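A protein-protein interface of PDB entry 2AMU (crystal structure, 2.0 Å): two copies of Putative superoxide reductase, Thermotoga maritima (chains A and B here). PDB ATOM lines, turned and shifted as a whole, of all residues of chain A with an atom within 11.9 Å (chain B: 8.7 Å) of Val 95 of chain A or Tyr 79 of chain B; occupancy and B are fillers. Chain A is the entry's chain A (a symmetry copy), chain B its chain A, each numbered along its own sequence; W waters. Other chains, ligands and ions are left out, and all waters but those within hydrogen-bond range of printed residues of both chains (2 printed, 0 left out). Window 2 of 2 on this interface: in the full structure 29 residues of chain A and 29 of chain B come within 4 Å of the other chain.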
ATOM      1  N   THR A  61     -35.717   5.767 -15.369  1.00  0.00           N
ATOM      2  CA  THR A  61     -35.617   4.311 -15.318  1.00  0.00           C
ATOM      3  C   THR A  61     -36.724   3.690 -16.206  1.00  0.00           C
ATOM      4  O   THR A  61     -36.496   2.684 -16.897  1.00  0.00           O
ATOM      5  CB  THR A  61     -35.706   3.806 -13.856  1.00  0.00           C
ATOM      6  OG1 THR A  61     -34.625   4.375 -13.089  1.00  0.00           O
ATOM      7  CG2 THR A  61     -35.673   2.282 -13.806  1.00  0.00           C
ATOM      8  N   ALA A  90     -27.235   3.391 -18.435  1.00  0.00           N
ATOM      9  CA  ALA A  90     -27.490   3.819 -17.105  1.00  0.00           C
ATOM     10  C   ALA A  90     -28.648   4.863 -17.173  1.00  0.00           C
ATOM     11  O   ALA A  90     -28.598   5.830 -17.934  1.00  0.00           O
ATOM     12  CB  ALA A  90     -26.222   4.406 -16.522  1.00  0.00           C
ATOM     13  N   HIS A  91     -29.695   4.640 -16.394  1.00  0.00           N
ATOM     14  CA  HIS A  91     -30.873   5.538 -16.356  1.00  0.00           C
ATOM     15  C   HIS A  91     -31.420   5.675 -14.919  1.00  0.00           C
ATOM     16  O   HIS A  91     -32.630   5.659 -14.700  1.00  0.00           O
ATOM     17  CB  HIS A  91     -31.960   4.996 -17.304  1.00  0.00           C
ATOM     18  CG  HIS A  91     -31.433   4.497 -18.626  1.00  0.00           C
ATOM     19  ND1 HIS A  91     -31.164   5.345 -19.687  1.00  0.00           N
ATOM     20  CD2 HIS A  91     -31.115   3.246 -19.051  1.00  0.00           C
ATOM     21  CE1 HIS A  91     -30.732   4.635 -20.720  1.00  0.00           C
ATOM     22  NE2 HIS A  91     -30.661   3.361 -20.351  1.00  0.00           N
ATOM     23  N   GLY A  92     -30.523   5.841 -13.947  1.00  0.00           N
ATOM     24  CA  GLY A  92     -30.909   6.120 -12.567  1.00  0.00           C
ATOM     25  C   GLY A  92     -31.490   4.984 -11.752  1.00  0.00           C
ATOM     26  O   GLY A  92     -32.002   5.211 -10.664  1.00  0.00           O
ATOM     27  N   GLU A  93     -31.412   3.764 -12.270  1.00  0.00           N
ATOM     28  CA  GLU A  93     -31.780   2.534 -11.532  1.00  0.00           C
ATOM     29  C   GLU A  93     -30.935   2.390 -10.259  1.00  0.00           C
ATOM     30  O   GLU A  93     -29.734   2.631 -10.292  1.00  0.00           O
ATOM     31  CB  GLU A  93     -31.433   1.301 -12.371  1.00  0.00           C
ATOM     32  CG  GLU A  93     -31.980   1.286 -13.739  1.00  0.00           C
ATOM     33  CD  GLU A  93     -31.169   2.022 -14.782  1.00  0.00           C
ATOM     34  OE1 GLU A  93     -29.958   2.292 -14.618  1.00  0.00           O
ATOM     35  OE2 GLU A  93     -31.781   2.312 -15.824  1.00  0.00           O
ATOM     36  N   SER A  94     -31.543   1.922  -9.179  1.00  0.00           N
ATOM     37  CA  SER A  94     -30.814   1.637  -7.969  1.00  0.00           C
ATOM     38  C   SER A  94     -31.545   0.588  -7.113  1.00  0.00           C
ATOM     39  O   SER A  94     -32.779   0.434  -7.206  1.00  0.00           O
ATOM     40  CB  SER A  94     -30.663   2.937  -7.150  1.00  0.00           C
ATOM     41  OG  SER A  94     -30.054   2.689  -5.898  1.00  0.00           O
ATOM     42  N   VAL A  95     -30.788  -0.080  -6.231  1.00  0.00           N
ATOM     43  CA  VAL A  95     -31.392  -0.897  -5.182  1.00  0.00           C
ATOM     44  C   VAL A  95     -32.267  -0.003  -4.272  1.00  0.00           C
ATOM     45  O   VAL A  95     -33.182  -0.504  -3.625  1.00  0.00           O
ATOM     46  CB  VAL A  95     -30.332  -1.700  -4.331  1.00  0.00           C
ATOM     47  CG1 VAL A  95     -29.448  -2.576  -5.216  1.00  0.00           C
ATOM     48  CG2 VAL A  95     -29.463  -0.787  -3.483  1.00  0.00           C
ATOM     49  N   GLN A  96     -32.001   1.307  -4.210  1.00  0.00           N
ATOM     50  CA  GLN A  96     -32.843   2.219  -3.405  1.00  0.00           C
ATOM     51  C   GLN A  96     -34.183   2.540  -4.086  1.00  0.00           C
ATOM     52  O   GLN A  96     -35.096   3.051  -3.457  1.00  0.00           O
ATOM     53  CB  GLN A  96     -32.101   3.524  -3.132  1.00  0.00           C
ATOM     54  CG  GLN A  96     -30.728   3.350  -2.514  1.00  0.00           C
ATOM     55  CD  GLN A  96     -30.781   2.844  -1.086  1.00  0.00           C
ATOM     56  OE1 GLN A  96     -31.769   3.038  -0.368  1.00  0.00           O
ATOM     57  NE2 GLN A  96     -29.688   2.222  -0.650  1.00  0.00           N
ATOM     58  N   GLY A  97     -34.291   2.256  -5.373  1.00  0.00           N
ATOM     59  CA  GLY A  97     -35.529   2.477  -6.145  1.00  0.00           C
ATOM     60  C   GLY A  97     -35.220   3.121  -7.492  1.00  0.00           C
ATOM     61  O   GLY A  97     -34.102   3.588  -7.756  1.00  0.00           O
ATOM     62  N   PRO A  98     -36.226   3.182  -8.363  1.00  0.00           N
ATOM     63  CA  PRO A  98     -36.012   3.773  -9.671  1.00  0.00           C
ATOM     64  C   PRO A  98     -35.742   5.271  -9.566  1.00  0.00           C
ATOM     65  O   PRO A  98     -36.290   5.911  -8.701  1.00  0.00           O
ATOM     66  CB  PRO A  98     -37.325   3.514 -10.400  1.00  0.00           C
ATOM     67  CG  PRO A  98     -38.335   3.348  -9.322  1.00  0.00           C
ATOM     68  CD  PRO A  98     -37.626   2.763  -8.150  1.00  0.00           C
ATOM     69  N   ASN A  99     -34.895   5.783 -10.456  1.00  0.00           N
ATOM     70  CA  ASN A  99     -34.491   7.191 -10.531  1.00  0.00           C
ATOM     71  C   ASN A  99     -33.805   7.752  -9.285  1.00  0.00           C
ATOM     72  O   ASN A  99     -33.800   8.967  -9.114  1.00  0.00           O
ATOM     73  CB  ASN A  99     -35.697   8.052 -10.923  1.00  0.00           C
ATOM     74  CG  ASN A  99     -36.393   7.528 -12.156  1.00  0.00           C
ATOM     75  OD1 ASN A  99     -35.783   7.437 -13.213  1.00  0.00           O
ATOM     76  ND2 ASN A  99     -37.663   7.122 -12.014  1.00  0.00           N
ATOM     77  N   ILE A 100     -33.257   6.874  -8.422  1.00  0.00           N
ATOM     78  CA  ILE A 100     -32.492   7.267  -7.188  1.00  0.00           C
ATOM     79  C   ILE A 100     -30.955   7.056  -7.434  1.00  0.00           C
ATOM     80  O   ILE A 100     -30.118   7.459  -6.622  1.00  0.00           O
ATOM     81  CB  ILE A 100     -33.028   6.513  -5.917  1.00  0.00           C
ATOM     82  CG1 ILE A 100     -34.483   6.893  -5.681  1.00  0.00           C
ATOM     83  CG2 ILE A 100     -32.318   6.896  -4.628  1.00  0.00           C
ATOM     84  CD1 ILE A 100     -35.110   6.152  -4.561  1.00  0.00           C
ATOM     85  N   GLY A 101     -30.619   6.456  -8.574  1.00  0.00           N
ATOM     86  CA  GLY A 101     -29.241   6.149  -8.968  1.00  0.00           C
ATOM     87  C   GLY A 101     -28.309   7.330  -9.264  1.00  0.00           C
ATOM     88  O   GLY A 101     -28.743   8.493  -9.352  1.00  0.00           O
ATOM     89  N   ALA A 102     -27.024   7.012  -9.408  1.00  0.00           N
ATOM     90  CA  ALA A 102     -25.960   7.997  -9.397  1.00  0.00           C
ATOM     91  C   ALA A 102     -25.619   8.488 -10.815  1.00  0.00           C
ATOM     92  O   ALA A 102     -24.956   9.504 -10.962  1.00  0.00           O
ATOM     93  CB  ALA A 102     -24.723   7.417  -8.733  1.00  0.00           C
ATOM     94  N   VAL A 103     -26.103   7.799 -11.847  1.00  0.00           N
ATOM     95  CA  VAL A 103     -25.604   7.977 -13.207  1.00  0.00           C
ATOM     96  C   VAL A 103     -26.676   7.744 -14.273  1.00  0.00           C
ATOM     97  O   VAL A 103     -27.463   6.831 -14.189  1.00  0.00           O
ATOM     98  CB  VAL A 103     -24.311   7.121 -13.500  1.00  0.00           C
ATOM     99  CG1 VAL A 103     -24.489   5.666 -13.116  1.00  0.00           C
ATOM    100  CG2 VAL A 103     -23.891   7.262 -14.962  1.00  0.00           C
ATOM    101  N   TYR A 104     -26.664   8.625 -15.269  1.00  0.00           N
ATOM    102  CA  TYR A 104     -27.569   8.627 -16.410  1.00  0.00           C
ATOM    103  C   TYR A 104     -26.691   8.787 -17.648  1.00  0.00           C
ATOM    104  O   TYR A 104     -25.822   9.686 -17.664  1.00  0.00           O
ATOM    105  CB  TYR A 104     -28.495   9.835 -16.346  1.00  0.00           C
ATOM    106  CG  TYR A 104     -29.502   9.765 -15.240  1.00  0.00           C
ATOM    107  CD1 TYR A 104     -29.160  10.093 -13.962  1.00  0.00           C
ATOM    108  CD2 TYR A 104     -30.768   9.303 -15.470  1.00  0.00           C
ATOM    109  CE1 TYR A 104     -30.080  10.011 -12.950  1.00  0.00           C
ATOM    110  CE2 TYR A 104     -31.707   9.202 -14.434  1.00  0.00           C
ATOM    111  CZ  TYR A 104     -31.355   9.550 -13.200  1.00  0.00           C
ATOM    112  OH  TYR A 104     -32.269   9.445 -12.162  1.00  0.00           O
ATOM    113  N   PHE B  71     -17.865   1.863 -17.409  1.00  0.00           N
ATOM    114  CA  PHE B  71     -18.535   1.617 -16.142  1.00  0.00           C
ATOM    115  C   PHE B  71     -18.360   2.789 -15.203  1.00  0.00           C
ATOM    116  O   PHE B  71     -17.331   3.495 -15.256  1.00  0.00           O
ATOM    117  CB  PHE B  71     -17.950   0.361 -15.475  1.00  0.00           C
ATOM    118  CG  PHE B  71     -18.300  -0.941 -16.202  1.00  0.00           C
ATOM    119  CD1 PHE B  71     -19.487  -1.559 -15.971  1.00  0.00           C
ATOM    120  CD2 PHE B  71     -17.418  -1.518 -17.103  1.00  0.00           C
ATOM    121  CE1 PHE B  71     -19.824  -2.721 -16.600  1.00  0.00           C
ATOM    122  CE2 PHE B  71     -17.750  -2.669 -17.723  1.00  0.00           C
ATOM    123  CZ  PHE B  71     -18.960  -3.271 -17.465  1.00  0.00           C
ATOM    124  N   PHE B  72     -19.359   2.993 -14.347  1.00  0.00           N
ATOM    125  CA  PHE B  72     -19.254   3.951 -13.240  1.00  0.00           C
ATOM    126  C   PHE B  72     -19.426   3.220 -11.935  1.00  0.00           C
ATOM    127  O   PHE B  72     -20.363   2.420 -11.757  1.00  0.00           O
ATOM    128  CB  PHE B  72     -20.279   5.074 -13.363  1.00  0.00           C
ATOM    129  CG  PHE B  72     -20.107   6.154 -12.344  1.00  0.00           C
ATOM    130  CD1 PHE B  72     -19.002   6.985 -12.377  1.00  0.00           C
ATOM    131  CD2 PHE B  72     -21.063   6.361 -11.364  1.00  0.00           C
ATOM    132  CE1 PHE B  72     -18.839   8.020 -11.420  1.00  0.00           C
ATOM    133  CE2 PHE B  72     -20.911   7.378 -10.422  1.00  0.00           C
ATOM    134  CZ  PHE B  72     -19.781   8.204 -10.454  1.00  0.00           C
ATOM    135  N   GLN B  73     -18.510   3.513 -11.022  1.00  0.00           N
ATOM    136  CA  GLN B  73     -18.524   2.969  -9.688  1.00  0.00           C
ATOM    137  C   GLN B  73     -18.741   4.118  -8.712  1.00  0.00           C
ATOM    138  O   GLN B  73     -17.805   4.871  -8.438  1.00  0.00           O
ATOM    139  CB  GLN B  73     -17.200   2.260  -9.398  1.00  0.00           C
ATOM    140  CG  GLN B  73     -17.288   1.164  -8.372  1.00  0.00           C
ATOM    141  CD  GLN B  73     -17.547   1.688  -7.006  1.00  0.00           C
ATOM    142  OE1 GLN B  73     -16.773   2.487  -6.495  1.00  0.00           O
ATOM    143  NE2 GLN B  73     -18.653   1.257  -6.397  1.00  0.00           N
ATOM    144  N   PRO B  74     -19.976   4.266  -8.189  1.00  0.00           N
ATOM    145  CA  PRO B  74     -20.230   5.375  -7.301  1.00  0.00           C
ATOM    146  C   PRO B  74     -19.512   5.149  -5.993  1.00  0.00           C
ATOM    147  O   PRO B  74     -19.577   4.036  -5.480  1.00  0.00           O
ATOM    148  CB  PRO B  74     -21.761   5.361  -7.119  1.00  0.00           C
ATOM    149  CG  PRO B  74     -22.308   4.430  -8.141  1.00  0.00           C
ATOM    150  CD  PRO B  74     -21.185   3.460  -8.456  1.00  0.00           C
ATOM    151  N   ASP B  75     -18.806   6.158  -5.468  1.00  0.00           N
ATOM    152  CA  ASP B  75     -18.066   5.993  -4.187  1.00  0.00           C
ATOM    153  C   ASP B  75     -19.049   5.539  -3.095  1.00  0.00           C
ATOM    154  O   ASP B  75     -20.123   6.123  -2.962  1.00  0.00           O
ATOM    155  CB  ASP B  75     -17.466   7.299  -3.658  1.00  0.00           C
ATOM    156  CG  ASP B  75     -16.321   7.830  -4.475  1.00  0.00           C
ATOM    157  OD1 ASP B  75     -15.666   7.086  -5.199  1.00  0.00           O
ATOM    158  OD2 ASP B  75     -16.061   9.037  -4.337  1.00  0.00           O
ATOM    159  N   GLY B  76     -18.674   4.511  -2.329  1.00  0.00           N
ATOM    160  CA  GLY B  76     -19.534   3.977  -1.289  1.00  0.00           C
ATOM    161  C   GLY B  76     -20.653   3.039  -1.750  1.00  0.00           C
ATOM    162  O   GLY B  76     -21.376   2.492  -0.915  1.00  0.00           O
ATOM    163  N   ASP B  77     -20.800   2.844  -3.057  1.00  0.00           N
ATOM    164  CA  ASP B  77     -21.715   1.859  -3.589  1.00  0.00           C
ATOM    165  C   ASP B  77     -20.982   0.506  -3.704  1.00  0.00           C
ATOM    166  O   ASP B  77     -19.774   0.475  -3.961  1.00  0.00           O
ATOM    167  CB  ASP B  77     -22.246   2.323  -4.939  1.00  0.00           C
ATOM    168  CG  ASP B  77     -23.570   1.688  -5.315  1.00  0.00           C
ATOM    169  OD1 ASP B  77     -24.613   2.259  -4.980  1.00  0.00           O
ATOM    170  OD2 ASP B  77     -23.583   0.627  -5.981  1.00  0.00           O
ATOM    171  N   PRO B  78     -21.702  -0.610  -3.467  1.00  0.00           N
ATOM    172  CA  PRO B  78     -21.143  -1.940  -3.657  1.00  0.00           C
ATOM    173  C   PRO B  78     -20.980  -2.379  -5.110  1.00  0.00           C
ATOM    174  O   PRO B  78     -20.293  -3.369  -5.355  1.00  0.00           O
ATOM    175  CB  PRO B  78     -22.156  -2.865  -2.976  1.00  0.00           C
ATOM    176  CG  PRO B  78     -23.144  -1.997  -2.272  1.00  0.00           C
ATOM    177  CD  PRO B  78     -23.080  -0.666  -2.952  1.00  0.00           C
ATOM    178  N   TYR B  79     -21.572  -1.672  -6.076  1.00  0.00           N
ATOM    179  CA  TYR B  79     -21.628  -2.171  -7.430  1.00  0.00           C
ATOM    180  C   TYR B  79     -20.968  -1.244  -8.464  1.00  0.00           C
ATOM    181  O   TYR B  79     -20.556  -0.131  -8.132  1.00  0.00           O
ATOM    182  CB  TYR B  79     -23.080  -2.418  -7.790  1.00  0.00           C
ATOM    183  CG  TYR B  79     -23.854  -3.252  -6.782  1.00  0.00           C
ATOM    184  CD1 TYR B  79     -23.582  -4.614  -6.605  1.00  0.00           C
ATOM    185  CD2 TYR B  79     -24.887  -2.696  -6.041  1.00  0.00           C
ATOM    186  CE1 TYR B  79     -24.292  -5.376  -5.682  1.00  0.00           C
ATOM    187  CE2 TYR B  79     -25.611  -3.457  -5.114  1.00  0.00           C
ATOM    188  CZ  TYR B  79     -25.314  -4.801  -4.950  1.00  0.00           C
ATOM    189  OH  TYR B  79     -26.030  -5.537  -4.031  1.00  0.00           O
ATOM    190  N   VAL B  80     -20.808  -1.755  -9.689  1.00  0.00           N
ATOM    191  CA  VAL B  80     -20.472  -0.954 -10.856  1.00  0.00           C
ATOM    192  C   VAL B  80     -21.731  -0.937 -11.704  1.00  0.00           C
ATOM    193  O   VAL B  80     -22.563  -1.859 -11.629  1.00  0.00           O
ATOM    194  CB  VAL B  80     -19.274  -1.470 -11.782  1.00  0.00           C
ATOM    195  CG1 VAL B  80     -17.930  -1.073 -11.244  1.00  0.00           C
ATOM    196  CG2 VAL B  80     -19.378  -2.985 -12.101  1.00  0.00           C
ATOM    197  N   TYR B  81     -21.855   0.120 -12.504  1.00  0.00           N
ATOM    198  CA  TYR B  81     -22.988   0.341 -13.377  1.00  0.00           C
ATOM    199  C   TYR B  81     -22.416   0.505 -14.784  1.00  0.00           C
ATOM    200  O   TYR B  81     -21.404   1.217 -15.007  1.00  0.00           O
ATOM    201  CB  TYR B  81     -23.866   1.549 -12.897  1.00  0.00           C
ATOM    202  CG  TYR B  81     -24.353   1.331 -11.491  1.00  0.00           C
ATOM    203  CD1 TYR B  81     -25.506   0.590 -11.231  1.00  0.00           C
ATOM    204  CD2 TYR B  81     -23.621   1.777 -10.406  1.00  0.00           C
ATOM    205  CE1 TYR B  81     -25.923   0.340  -9.943  1.00  0.00           C
ATOM    206  CE2 TYR B  81     -24.050   1.516  -9.103  1.00  0.00           C
ATOM    207  CZ  TYR B  81     -25.205   0.794  -8.890  1.00  0.00           C
ATOM    208  OH  TYR B  81     -25.645   0.517  -7.604  1.00  0.00           O
ATOM    209  N   GLU B  82     -23.034  -0.196 -15.728  1.00  0.00           N
ATOM    210  CA  GLU B  82     -22.637  -0.091 -17.111  1.00  0.00           C
ATOM    211  C   GLU B  82     -23.183   1.199 -17.696  1.00  0.00           C
ATOM    212  O   GLU B  82     -24.366   1.305 -17.970  1.00  0.00           O
ATOM    213  CB  GLU B  82     -23.129  -1.295 -17.906  1.00  0.00           C
ATOM    214  CG  GLU B  82     -22.553  -1.356 -19.322  1.00  0.00           C
ATOM    215  CD  GLU B  82     -22.959  -2.616 -20.116  1.00  0.00           C
ATOM    216  OE1 GLU B  82     -24.149  -2.772 -20.477  1.00  0.00           O
ATOM    217  OE2 GLU B  82     -22.045  -3.413 -20.430  1.00  0.00           O
ATOM    218  N   ARG B 117     -23.063  11.874  -7.985  1.00  0.00           N
ATOM    219  CA  ARG B 117     -22.176  11.421  -6.933  1.00  0.00           C
ATOM    220  C   ARG B 117     -20.782  11.161  -7.464  1.00  0.00           C
ATOM    221  O   ARG B 117     -20.632  10.679  -8.557  1.00  0.00           O
ATOM    222  CB  ARG B 117     -22.696  10.124  -6.335  1.00  0.00           C
ATOM    223  CG  ARG B 117     -22.109   9.888  -4.973  1.00  0.00           C
ATOM    224  CD  ARG B 117     -22.225   8.479  -4.569  1.00  0.00           C
ATOM    225  NE  ARG B 117     -23.569   7.971  -4.789  1.00  0.00           N
ATOM    226  CZ  ARG B 117     -23.965   6.798  -4.318  1.00  0.00           C
ATOM    227  NH1 ARG B 117     -23.120   6.040  -3.573  1.00  0.00           N
ATOM    228  NH2 ARG B 117     -25.216   6.401  -4.561  1.00  0.00           N
ATOM    229  N   THR B 120     -15.782   6.482  -9.710  1.00  0.00           N
ATOM    230  CA  THR B 120     -14.680   6.101 -10.594  1.00  0.00           C
ATOM    231  C   THR B 120     -15.203   5.685 -11.978  1.00  0.00           C
ATOM    232  O   THR B 120     -16.122   4.851 -12.091  1.00  0.00           O
ATOM    233  CB  THR B 120     -13.888   4.939 -10.037  1.00  0.00           C
ATOM    234  OG1 THR B 120     -13.466   5.259  -8.710  1.00  0.00           O
ATOM    235  CG2 THR B 120     -12.678   4.631 -10.919  1.00  0.00           C
ATOM    236  N   ILE B 122     -14.525   3.565 -15.131  1.00  0.00           N
ATOM    237  CA  ILE B 122     -13.723   2.391 -15.541  1.00  0.00           C
ATOM    238  C   ILE B 122     -13.997   2.136 -17.034  1.00  0.00           C
ATOM    239  O   ILE B 122     -15.152   2.003 -17.443  1.00  0.00           O
ATOM    240  CB  ILE B 122     -14.009   1.102 -14.689  1.00  0.00           C
ATOM    241  CG1 ILE B 122     -13.862   1.415 -13.185  1.00  0.00           C
ATOM    242  CG2 ILE B 122     -13.116  -0.073 -15.193  1.00  0.00           C
ATOM    243  CD1 ILE B 122     -14.148   0.222 -12.177  1.00  0.00           C
HETATM  244  O   HOH W   1     -28.004  -0.482  -6.974  1.00  0.00           O
HETATM  245  O   HOH W   2     -27.039   8.776  -5.947  1.00  0.00           O
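The backbone carbonyl oxygen of Tyr 81 of chain B is in hydrogen-bond range of the backbone NH of Phe 72 of chain B (2.8 Å). NE2 of Gln 73 of chain B is in hydrogen-bond range of O of Tyr 79 of chain B (2.9 Å). The side-chain carboxylate of Asp 77 of chain B sits at hydrogen-bond distance from the backbone NH of Tyr 79 of chain B (3.1 Å). The backbone carbonyl oxygen (O) of Val 103 of chain A is in hydrogen-bond range of the backbone NH (N) of Gly 92 of chain A (3.2 Å).
O of Glu 82 of chain B touches N of Ala 90 of chain A (3.6 Å). Tyr 79 of chain B touches Val 95 of chain A. Ala 102 of chain A touches Pro 74 of chain B. CD2 of Phe 72 of chain B touches CG1 of Val 103 of chain A (3.9 Å).
Of the printed residues of chain B, Ala 90 of chain A touches Glu 82 (3.6 Å). No residue of chain B comes within 4 Å of Ser 94 of chain A. Val 95 of chain A touches just one residue of chain B: Tyr 79. Asn 99 of chain A touches none of the printed residues of chain B. Of the printed residues of chain B, Ala 102 of chain A touches Pro 74 (3.9 Å). Of the printed residues of chain B, Val 103 of chain A touches Phe 72 (3.9 Å). No residue of chain A comes within 4 Å of Gly 76 of chain B. No residue of chain A comes within 4 Å of Pro 78 of chain B. Tyr 79 of chain B touches just one residue of chain A: Val 95 (3.9 Å). Ile 122 of chain B touches none of the printed residues of chain A. The nearest residue of chain A that does not touch Tyr 79 of chain B is Ser 94 of chain A (7.5 Å). The nearest printed residue of chain B that does not touch Ala 102 of chain A is Arg 117 of chain B (4.1 Å).
Of the 15 printed residues of chain B, 4 touch a printed residue of chain A. Printed residues of chain B that touch a printed residue of chain A: Phe 72, Pro 74, Tyr 79 and Glu 82. Among the printed residues, 4 pairs touch across the chains.
No position is printed for both chains. Of the 4 pairs that touch across the chains among the printed residues, none has its exchanged pair printed and touching as well.
Water W1 lies within hydrogen-bond range of the side-chain hydroxyl of Tyr 81 of chain B and the backbone NH of Val 95 of chain A. Water W2 bridges NH2 of Arg 117 of chain B (3.3 Å) and O of Ile 100 of chain A (3.4 Å).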
